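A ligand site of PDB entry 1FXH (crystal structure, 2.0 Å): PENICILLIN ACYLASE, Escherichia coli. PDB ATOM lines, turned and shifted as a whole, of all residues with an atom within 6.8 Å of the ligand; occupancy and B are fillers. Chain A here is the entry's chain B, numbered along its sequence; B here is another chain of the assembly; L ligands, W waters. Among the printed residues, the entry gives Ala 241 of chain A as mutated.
O2 of the ligand lies within hydrogen-bond range of OG of Ser 1, 2.7 Å away. N of Ala 69 is in hydrogen-bond range of O2 of the ligand (3.0 Å).
The side-chain hydroxyl (OG) of Ser 1 sits at hydrogen-bond distance from the backbone NH (N) of Gln 23, 2.6 Å away. O of Ala 69 is in hydrogen-bond range of ND2 of Asn 178 (3.2 Å). O of Asn 178 lies close to OG of Ser 67. The backbone NH of Ser 67 is in hydrogen-bond range of the side-chain amide oxygen of Asn 20. The backbone NH of Asn 178 lies within hydrogen-bond range of the backbone carbonyl oxygen of Thr 68.
Merely in contact with the ligand: Phe 146 of chain B (3.2 Å), Phe 24 (3.4 Å), Thr 68 (3.5 Å), Ser 67 (3.5 Å), Met 142 of chain B (3.5 Å), Ile 177 (3.8 Å) and Gln 23 (3.8 Å). Hydrophobic or aromatic side chains within 4 Å of the ligand: Phe 24, Ala 69, Ile 177, Met 142 of chain B and Phe 146 of chain B. Of the 25 residues printed, 9 come within 4 Å of the ligand.
Water W3 bridges N of Ser 1 (2.8 Å) and O2 of the ligand (2.9 Å). Water W2 lies within hydrogen-bond range of the backbone NH of Ser 1 (2.9 Å), the backbone carbonyl oxygen of Gln 23 (3.0 Å) and an oxygen (O1) of the ligand (3.2 Å).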
ATOM      1  N   SER A   1       1.086  15.129  18.366  1.00  0.00           N
ATOM      2  CA  SER A   1       1.774  14.627  17.136  1.00  0.00           C
ATOM      3  C   SER A   1       3.276  14.555  17.387  1.00  0.00           C
ATOM      4  O   SER A   1       3.839  15.399  18.071  1.00  0.00           O
ATOM      5  CB  SER A   1       1.521  15.569  15.964  1.00  0.00           C
ATOM      6  OG  SER A   1       0.143  15.680  15.681  1.00  0.00           O
ATOM      7  N   ASN A   2       3.915  13.538  16.824  1.00  0.00           N
ATOM      8  CA  ASN A   2       5.368  13.476  16.929  1.00  0.00           C
ATOM      9  C   ASN A   2       6.065  13.371  15.587  1.00  0.00           C
ATOM     10  O   ASN A   2       5.460  13.108  14.553  1.00  0.00           O
ATOM     11  CB  ASN A   2       5.820  12.361  17.898  1.00  0.00           C
ATOM     12  CG  ASN A   2       5.243  10.987  17.548  1.00  0.00           C
ATOM     13  OD1 ASN A   2       5.064  10.153  18.442  1.00  0.00           O
ATOM     14  ND2 ASN A   2       4.995  10.737  16.279  1.00  0.00           N
ATOM     15  N   ASN A  20       7.176  10.683  10.717  1.00  0.00           N
ATOM     16  CA  ASN A  20       6.170  11.644  11.155  1.00  0.00           C
ATOM     17  C   ASN A  20       4.940  10.901  11.651  1.00  0.00           C
ATOM     18  O   ASN A  20       4.507   9.943  11.019  1.00  0.00           O
ATOM     19  CB  ASN A  20       5.802  12.548   9.969  1.00  0.00           C
ATOM     20  CG  ASN A  20       5.220  13.892  10.382  1.00  0.00           C
ATOM     21  OD1 ASN A  20       4.968  14.741   9.524  1.00  0.00           O
ATOM     22  ND2 ASN A  20       5.027  14.116  11.679  1.00  0.00           N
ATOM     23  N   GLY A  21       4.405  11.330  12.781  1.00  0.00           N
ATOM     24  CA  GLY A  21       3.207  10.696  13.319  1.00  0.00           C
ATOM     25  C   GLY A  21       2.241  11.743  13.799  1.00  0.00           C
ATOM     26  O   GLY A  21       2.089  11.955  15.003  1.00  0.00           O
ATOM     27  N   PRO A  22       1.554  12.436  12.874  1.00  0.00           N
ATOM     28  CA  PRO A  22       0.595  13.477  13.264  1.00  0.00           C
ATOM     29  C   PRO A  22      -0.565  12.819  13.992  1.00  0.00           C
ATOM     30  O   PRO A  22      -1.098  11.815  13.518  1.00  0.00           O
ATOM     31  CB  PRO A  22       0.178  14.067  11.930  1.00  0.00           C
ATOM     32  CG  PRO A  22       0.234  12.852  11.014  1.00  0.00           C
ATOM     33  CD  PRO A  22       1.543  12.224  11.412  1.00  0.00           C
ATOM     34  N   GLN A  23      -0.938  13.373  15.131  1.00  0.00           N
ATOM     35  CA  GLN A  23      -1.994  12.760  15.925  1.00  0.00           C
ATOM     36  C   GLN A  23      -3.260  13.606  15.939  1.00  0.00           C
ATOM     37  O   GLN A  23      -3.361  14.595  16.671  1.00  0.00           O
ATOM     38  CB  GLN A  23      -1.473  12.500  17.341  1.00  0.00           C
ATOM     39  CG  GLN A  23      -0.406  11.409  17.369  1.00  0.00           C
ATOM     40  CD  GLN A  23       0.151  11.170  18.749  1.00  0.00           C
ATOM     41  OE1 GLN A  23       0.885  11.992  19.285  1.00  0.00           O
ATOM     42  NE2 GLN A  23      -0.194  10.011  19.344  1.00  0.00           N
ATOM     43  N   PHE A  24      -4.218  13.192  15.123  1.00  0.00           N
ATOM     44  CA  PHE A  24      -5.466  13.919  14.902  1.00  0.00           C
ATOM     45  C   PHE A  24      -6.661  13.201  15.526  1.00  0.00           C
ATOM     46  O   PHE A  24      -7.801  13.672  15.428  1.00  0.00           O
ATOM     47  CB  PHE A  24      -5.741  14.031  13.402  1.00  0.00           C
ATOM     48  CG  PHE A  24      -4.699  14.766  12.640  1.00  0.00           C
ATOM     49  CD1 PHE A  24      -4.589  16.146  12.741  1.00  0.00           C
ATOM     50  CD2 PHE A  24      -3.852  14.084  11.764  1.00  0.00           C
ATOM     51  CE1 PHE A  24      -3.669  16.837  11.967  1.00  0.00           C
ATOM     52  CE2 PHE A  24      -2.933  14.775  10.990  1.00  0.00           C
ATOM     53  CZ  PHE A  24      -2.840  16.158  11.093  1.00  0.00           C
ATOM     54  N   TYR A  31      -8.477   9.929   8.233  1.00  0.00           N
ATOM     55  CA  TYR A  31      -8.348  11.361   8.420  1.00  0.00           C
ATOM     56  C   TYR A  31      -7.591  11.969   7.249  1.00  0.00           C
ATOM     57  O   TYR A  31      -7.911  13.075   6.801  1.00  0.00           O
ATOM     58  CB  TYR A  31      -7.597  11.667   9.702  1.00  0.00           C
ATOM     59  CG  TYR A  31      -7.650  13.119  10.099  1.00  0.00           C
ATOM     60  CD1 TYR A  31      -8.776  13.645  10.740  1.00  0.00           C
ATOM     61  CD2 TYR A  31      -6.573  13.979   9.855  1.00  0.00           C
ATOM     62  CE1 TYR A  31      -8.817  14.986  11.126  1.00  0.00           C
ATOM     63  CE2 TYR A  31      -6.616  15.315  10.227  1.00  0.00           C
ATOM     64  CZ  TYR A  31      -7.742  15.811  10.870  1.00  0.00           C
ATOM     65  OH  TYR A  31      -7.763  17.118  11.293  1.00  0.00           O
ATOM     66  N   PRO A  49      -4.380  15.664   5.354  1.00  0.00           N
ATOM     67  CA  PRO A  49      -5.700  15.731   5.991  1.00  0.00           C
ATOM     68  C   PRO A  49      -6.766  16.312   5.051  1.00  0.00           C
ATOM     69  O   PRO A  49      -6.507  17.296   4.352  1.00  0.00           O
ATOM     70  CB  PRO A  49      -5.463  16.629   7.207  1.00  0.00           C
ATOM     71  CG  PRO A  49      -4.005  16.400   7.515  1.00  0.00           C
ATOM     72  CD  PRO A  49      -3.387  16.423   6.138  1.00  0.00           C
ATOM     73  N   VAL A  56       0.493  17.816   3.541  1.00  0.00           N
ATOM     74  CA  VAL A  56       1.172  18.097   4.805  1.00  0.00           C
ATOM     75  C   VAL A  56       2.265  17.054   5.046  1.00  0.00           C
ATOM     76  O   VAL A  56       3.256  17.328   5.714  1.00  0.00           O
ATOM     77  CB  VAL A  56       0.187  18.082   5.999  1.00  0.00           C
ATOM     78  CG1 VAL A  56       0.921  18.442   7.289  1.00  0.00           C
ATOM     79  CG2 VAL A  56      -0.963  19.053   5.737  1.00  0.00           C
ATOM     80  N   PHE A  57       2.087  15.867   4.467  1.00  0.00           N
ATOM     81  CA  PHE A  57       3.046  14.774   4.664  1.00  0.00           C
ATOM     82  C   PHE A  57       3.467  14.177   3.321  1.00  0.00           C
ATOM     83  O   PHE A  57       2.661  13.542   2.632  1.00  0.00           O
ATOM     84  CB  PHE A  57       2.397  13.682   5.520  1.00  0.00           C
ATOM     85  CG  PHE A  57       1.640  14.217   6.698  1.00  0.00           C
ATOM     86  CD1 PHE A  57       2.318  14.838   7.742  1.00  0.00           C
ATOM     87  CD2 PHE A  57       0.258  14.152   6.741  1.00  0.00           C
ATOM     88  CE1 PHE A  57       1.624  15.389   8.807  1.00  0.00           C
ATOM     89  CE2 PHE A  57      -0.453  14.707   7.808  1.00  0.00           C
ATOM     90  CZ  PHE A  57       0.230  15.330   8.835  1.00  0.00           C
ATOM     91  N   GLY A  66       7.136  17.550   6.796  1.00  0.00           N
ATOM     92  CA  GLY A  66       6.154  17.054   7.737  1.00  0.00           C
ATOM     93  C   GLY A  66       5.767  18.154   8.705  1.00  0.00           C
ATOM     94  O   GLY A  66       6.356  19.240   8.679  1.00  0.00           O
ATOM     95  N   SER A  67       4.784  17.876   9.554  1.00  0.00           N
ATOM     96  CA  SER A  67       4.309  18.865  10.512  1.00  0.00           C
ATOM     97  C   SER A  67       3.871  18.238  11.833  1.00  0.00           C
ATOM     98  O   SER A  67       3.557  17.053  11.906  1.00  0.00           O
ATOM     99  CB  SER A  67       3.127  19.656   9.937  1.00  0.00           C
ATOM    100  OG  SER A  67       3.529  20.567   8.930  1.00  0.00           O
ATOM    101  N   THR A  68       3.868  19.061  12.879  1.00  0.00           N
ATOM    102  CA  THR A  68       3.212  18.760  14.139  1.00  0.00           C
ATOM    103  C   THR A  68       2.680  20.106  14.634  1.00  0.00           C
ATOM    104  O   THR A  68       3.249  21.135  14.291  1.00  0.00           O
ATOM    105  CB  THR A  68       4.181  18.170  15.196  1.00  0.00           C
ATOM    106  OG1 THR A  68       5.113  19.186  15.616  1.00  0.00           O
ATOM    107  CG2 THR A  68       4.956  16.986  14.618  1.00  0.00           C
ATOM    108  N   ALA A  69       1.609  20.104  15.417  1.00  0.00           N
ATOM    109  CA  ALA A  69       1.060  21.378  15.884  1.00  0.00           C
ATOM    110  C   ALA A  69       2.122  22.163  16.649  1.00  0.00           C
ATOM    111  O   ALA A  69       2.911  21.575  17.381  1.00  0.00           O
ATOM    112  CB  ALA A  69      -0.147  21.151  16.761  1.00  0.00           C
ATOM    113  N   GLY A  70       2.137  23.474  16.465  1.00  0.00           N
ATOM    114  CA  GLY A  70       3.143  24.313  17.093  1.00  0.00           C
ATOM    115  C   GLY A  70       2.830  24.659  18.536  1.00  0.00           C
ATOM    116  O   GLY A  70       3.725  24.690  19.379  1.00  0.00           O
ATOM    117  N   PHE A  71       1.558  24.925  18.832  1.00  0.00           N
ATOM    118  CA  PHE A  71       1.161  25.286  20.186  1.00  0.00           C
ATOM    119  C   PHE A  71       1.861  26.543  20.688  1.00  0.00           C
ATOM    120  O   PHE A  71       2.146  26.668  21.878  1.00  0.00           O
ATOM    121  CB  PHE A  71       1.447  24.134  21.157  1.00  0.00           C
ATOM    122  CG  PHE A  71       0.551  22.955  20.955  1.00  0.00           C
ATOM    123  CD1 PHE A  71      -0.786  23.006  21.330  1.00  0.00           C
ATOM    124  CD2 PHE A  71       1.039  21.793  20.365  1.00  0.00           C
ATOM    125  CE1 PHE A  71      -1.630  21.911  21.131  1.00  0.00           C
ATOM    126  CE2 PHE A  71       0.213  20.695  20.164  1.00  0.00           C
ATOM    127  CZ  PHE A  71      -1.121  20.759  20.541  1.00  0.00           C
ATOM    128  N   TRP A 154       1.455  25.976   2.140  1.00  0.00           N
ATOM    129  CA  TRP A 154       1.558  24.533   2.340  1.00  0.00           C
ATOM    130  C   TRP A 154       1.574  23.801   1.007  1.00  0.00           C
ATOM    131  O   TRP A 154       2.007  22.647   0.911  1.00  0.00           O
ATOM    132  CB  TRP A 154       0.367  24.031   3.165  1.00  0.00           C
ATOM    133  CG  TRP A 154       0.782  23.214   4.347  1.00  0.00           C
ATOM    134  CD1 TRP A 154       1.676  22.179   4.363  1.00  0.00           C
ATOM    135  CD2 TRP A 154       0.318  23.354   5.699  1.00  0.00           C
ATOM    136  NE1 TRP A 154       1.797  21.674   5.636  1.00  0.00           N
ATOM    137  CE2 TRP A 154       0.969  22.381   6.478  1.00  0.00           C
ATOM    138  CE3 TRP A 154      -0.599  24.220   6.325  1.00  0.00           C
ATOM    139  CZ2 TRP A 154       0.747  22.242   7.849  1.00  0.00           C
ATOM    140  CZ3 TRP A 154      -0.818  24.074   7.691  1.00  0.00           C
ATOM    141  CH2 TRP A 154      -0.147  23.096   8.438  1.00  0.00           C
ATOM    142  N   THR A 176       0.061  28.355  13.752  1.00  0.00           N
ATOM    143  CA  THR A 176       1.159  27.917  14.612  1.00  0.00           C
ATOM    144  C   THR A 176       1.437  26.428  14.407  1.00  0.00           C
ATOM    145  O   THR A 176       0.806  25.571  15.028  1.00  0.00           O
ATOM    146  CB  THR A 176       0.885  28.200  16.105  1.00  0.00           C
ATOM    147  OG1 THR A 176       1.944  27.639  16.883  1.00  0.00           O
ATOM    148  CG2 THR A 176      -0.449  27.616  16.545  1.00  0.00           C
ATOM    149  N   ILE A 177       2.394  26.150  13.528  1.00  0.00           N
ATOM    150  CA  ILE A 177       2.688  24.788  13.115  1.00  0.00           C
ATOM    151  C   ILE A 177       4.186  24.570  13.029  1.00  0.00           C
ATOM    152  O   ILE A 177       4.919  25.398  12.475  1.00  0.00           O
ATOM    153  CB  ILE A 177       2.103  24.512  11.721  1.00  0.00           C
ATOM    154  CG1 ILE A 177       0.630  24.924  11.659  1.00  0.00           C
ATOM    155  CG2 ILE A 177       2.263  23.033  11.375  1.00  0.00           C
ATOM    156  CD1 ILE A 177      -0.288  24.064  12.501  1.00  0.00           C
ATOM    157  N   ASN A 178       4.661  23.454  13.575  1.00  0.00           N
ATOM    158  CA  ASN A 178       6.042  23.076  13.349  1.00  0.00           C
ATOM    159  C   ASN A 178       6.143  22.427  11.991  1.00  0.00           C
ATOM    160  O   ASN A 178       5.369  21.505  11.666  1.00  0.00           O
ATOM    161  CB  ASN A 178       6.527  22.102  14.425  1.00  0.00           C
ATOM    162  CG  ASN A 178       6.532  22.709  15.801  1.00  0.00           C
ATOM    163  OD1 ASN A 178       7.002  23.838  15.983  1.00  0.00           O
ATOM    164  ND2 ASN A 178       6.010  21.977  16.786  1.00  0.00           N
ATOM    165  N   ALA A 241       5.052  17.716  20.406  1.00  0.00           N
ATOM    166  CA  ALA A 241       4.263  18.836  20.916  1.00  0.00           C
ATOM    167  C   ALA A 241       4.992  19.543  22.059  1.00  0.00           C
ATOM    168  O   ALA A 241       4.357  20.210  22.890  1.00  0.00           O
ATOM    169  CB  ALA A 241       2.889  18.367  21.378  1.00  0.00           C
ATOM    170  N   ARG A 263       7.009  14.447  27.222  1.00  0.00           N
ATOM    171  CA  ARG A 263       7.049  13.145  26.568  1.00  0.00           C
ATOM    172  C   ARG A 263       8.061  13.064  25.423  1.00  0.00           C
ATOM    173  O   ARG A 263       8.386  11.960  24.976  1.00  0.00           O
ATOM    174  CB  ARG A 263       5.662  12.776  26.041  1.00  0.00           C
ATOM    175  CG  ARG A 263       5.152  13.701  24.938  1.00  0.00           C
ATOM    176  CD  ARG A 263       3.708  13.409  24.569  1.00  0.00           C
ATOM    177  NE  ARG A 263       3.212  14.355  23.570  1.00  0.00           N
ATOM    178  CZ  ARG A 263       1.972  14.409  23.125  1.00  0.00           C
ATOM    179  NH1 ARG A 263       1.050  13.567  23.586  1.00  0.00           N
ATOM    180  NH2 ARG A 263       1.639  15.321  22.223  1.00  0.00           N
ATOM    181  N   MET B 142      -7.994  23.071  10.027  1.00  0.00           N
ATOM    182  CA  MET B 142      -6.598  23.273  10.388  1.00  0.00           C
ATOM    183  C   MET B 142      -6.431  24.570  11.167  1.00  0.00           C
ATOM    184  O   MET B 142      -5.854  24.578  12.248  1.00  0.00           O
ATOM    185  CB  MET B 142      -5.708  23.284   9.136  1.00  0.00           C
ATOM    186  CG  MET B 142      -4.214  23.400   9.411  1.00  0.00           C
ATOM    187  SD  MET B 142      -3.530  22.053  10.438  1.00  0.00           S
ATOM    188  CE  MET B 142      -3.208  20.789   9.217  1.00  0.00           C
ATOM    189  N   PHE B 146      -6.959  23.824  15.039  1.00  0.00           N
ATOM    190  CA  PHE B 146      -5.634  23.465  15.514  1.00  0.00           C
ATOM    191  C   PHE B 146      -4.738  24.674  15.781  1.00  0.00           C
ATOM    192  O   PHE B 146      -3.628  24.526  16.284  1.00  0.00           O
ATOM    193  CB  PHE B 146      -4.934  22.518  14.536  1.00  0.00           C
ATOM    194  CG  PHE B 146      -5.262  21.069  14.762  1.00  0.00           C
ATOM    195  CD1 PHE B 146      -5.000  20.468  15.990  1.00  0.00           C
ATOM    196  CD2 PHE B 146      -5.852  20.310  13.755  1.00  0.00           C
ATOM    197  CE1 PHE B 146      -5.322  19.135  16.216  1.00  0.00           C
ATOM    198  CE2 PHE B 146      -6.181  18.971  13.984  1.00  0.00           C
ATOM    199  CZ  PHE B 146      -5.912  18.377  15.209  1.00  0.00           C
HETATM  200  C1  LIG L   1      -1.528  18.159  16.424  1.00  0.00           C
HETATM  201  C2  LIG L   1      -2.209  17.867  15.103  1.00  0.00           C
HETATM  202  C3  LIG L   1      -1.423  18.466  13.945  1.00  0.00           C
HETATM  203  C4  LIG L   1      -0.350  17.801  13.282  1.00  0.00           C
HETATM  204  C5  LIG L   1       0.331  18.398  12.209  1.00  0.00           C
HETATM  205  C6  LIG L   1      -0.121  19.677  11.857  1.00  0.00           C
HETATM  206  C7  LIG L   1      -1.174  20.366  12.486  1.00  0.00           C
HETATM  207  C8  LIG L   1      -1.853  19.752  13.564  1.00  0.00           C
HETATM  208  O1  LIG L   1      -2.416  18.418  17.320  1.00  0.00           O
HETATM  209  O2  LIG L   1      -0.301  18.140  16.597  1.00  0.00           O
HETATM  210  O   HOH W   1      -4.066  19.013  19.983  1.00  0.00           O
HETATM  211  O   HOH W   2      -1.683  15.740  18.850  1.00  0.00           O
HETATM  212  O   HOH W   3       0.580  17.756  19.329  1.00  0.00           O
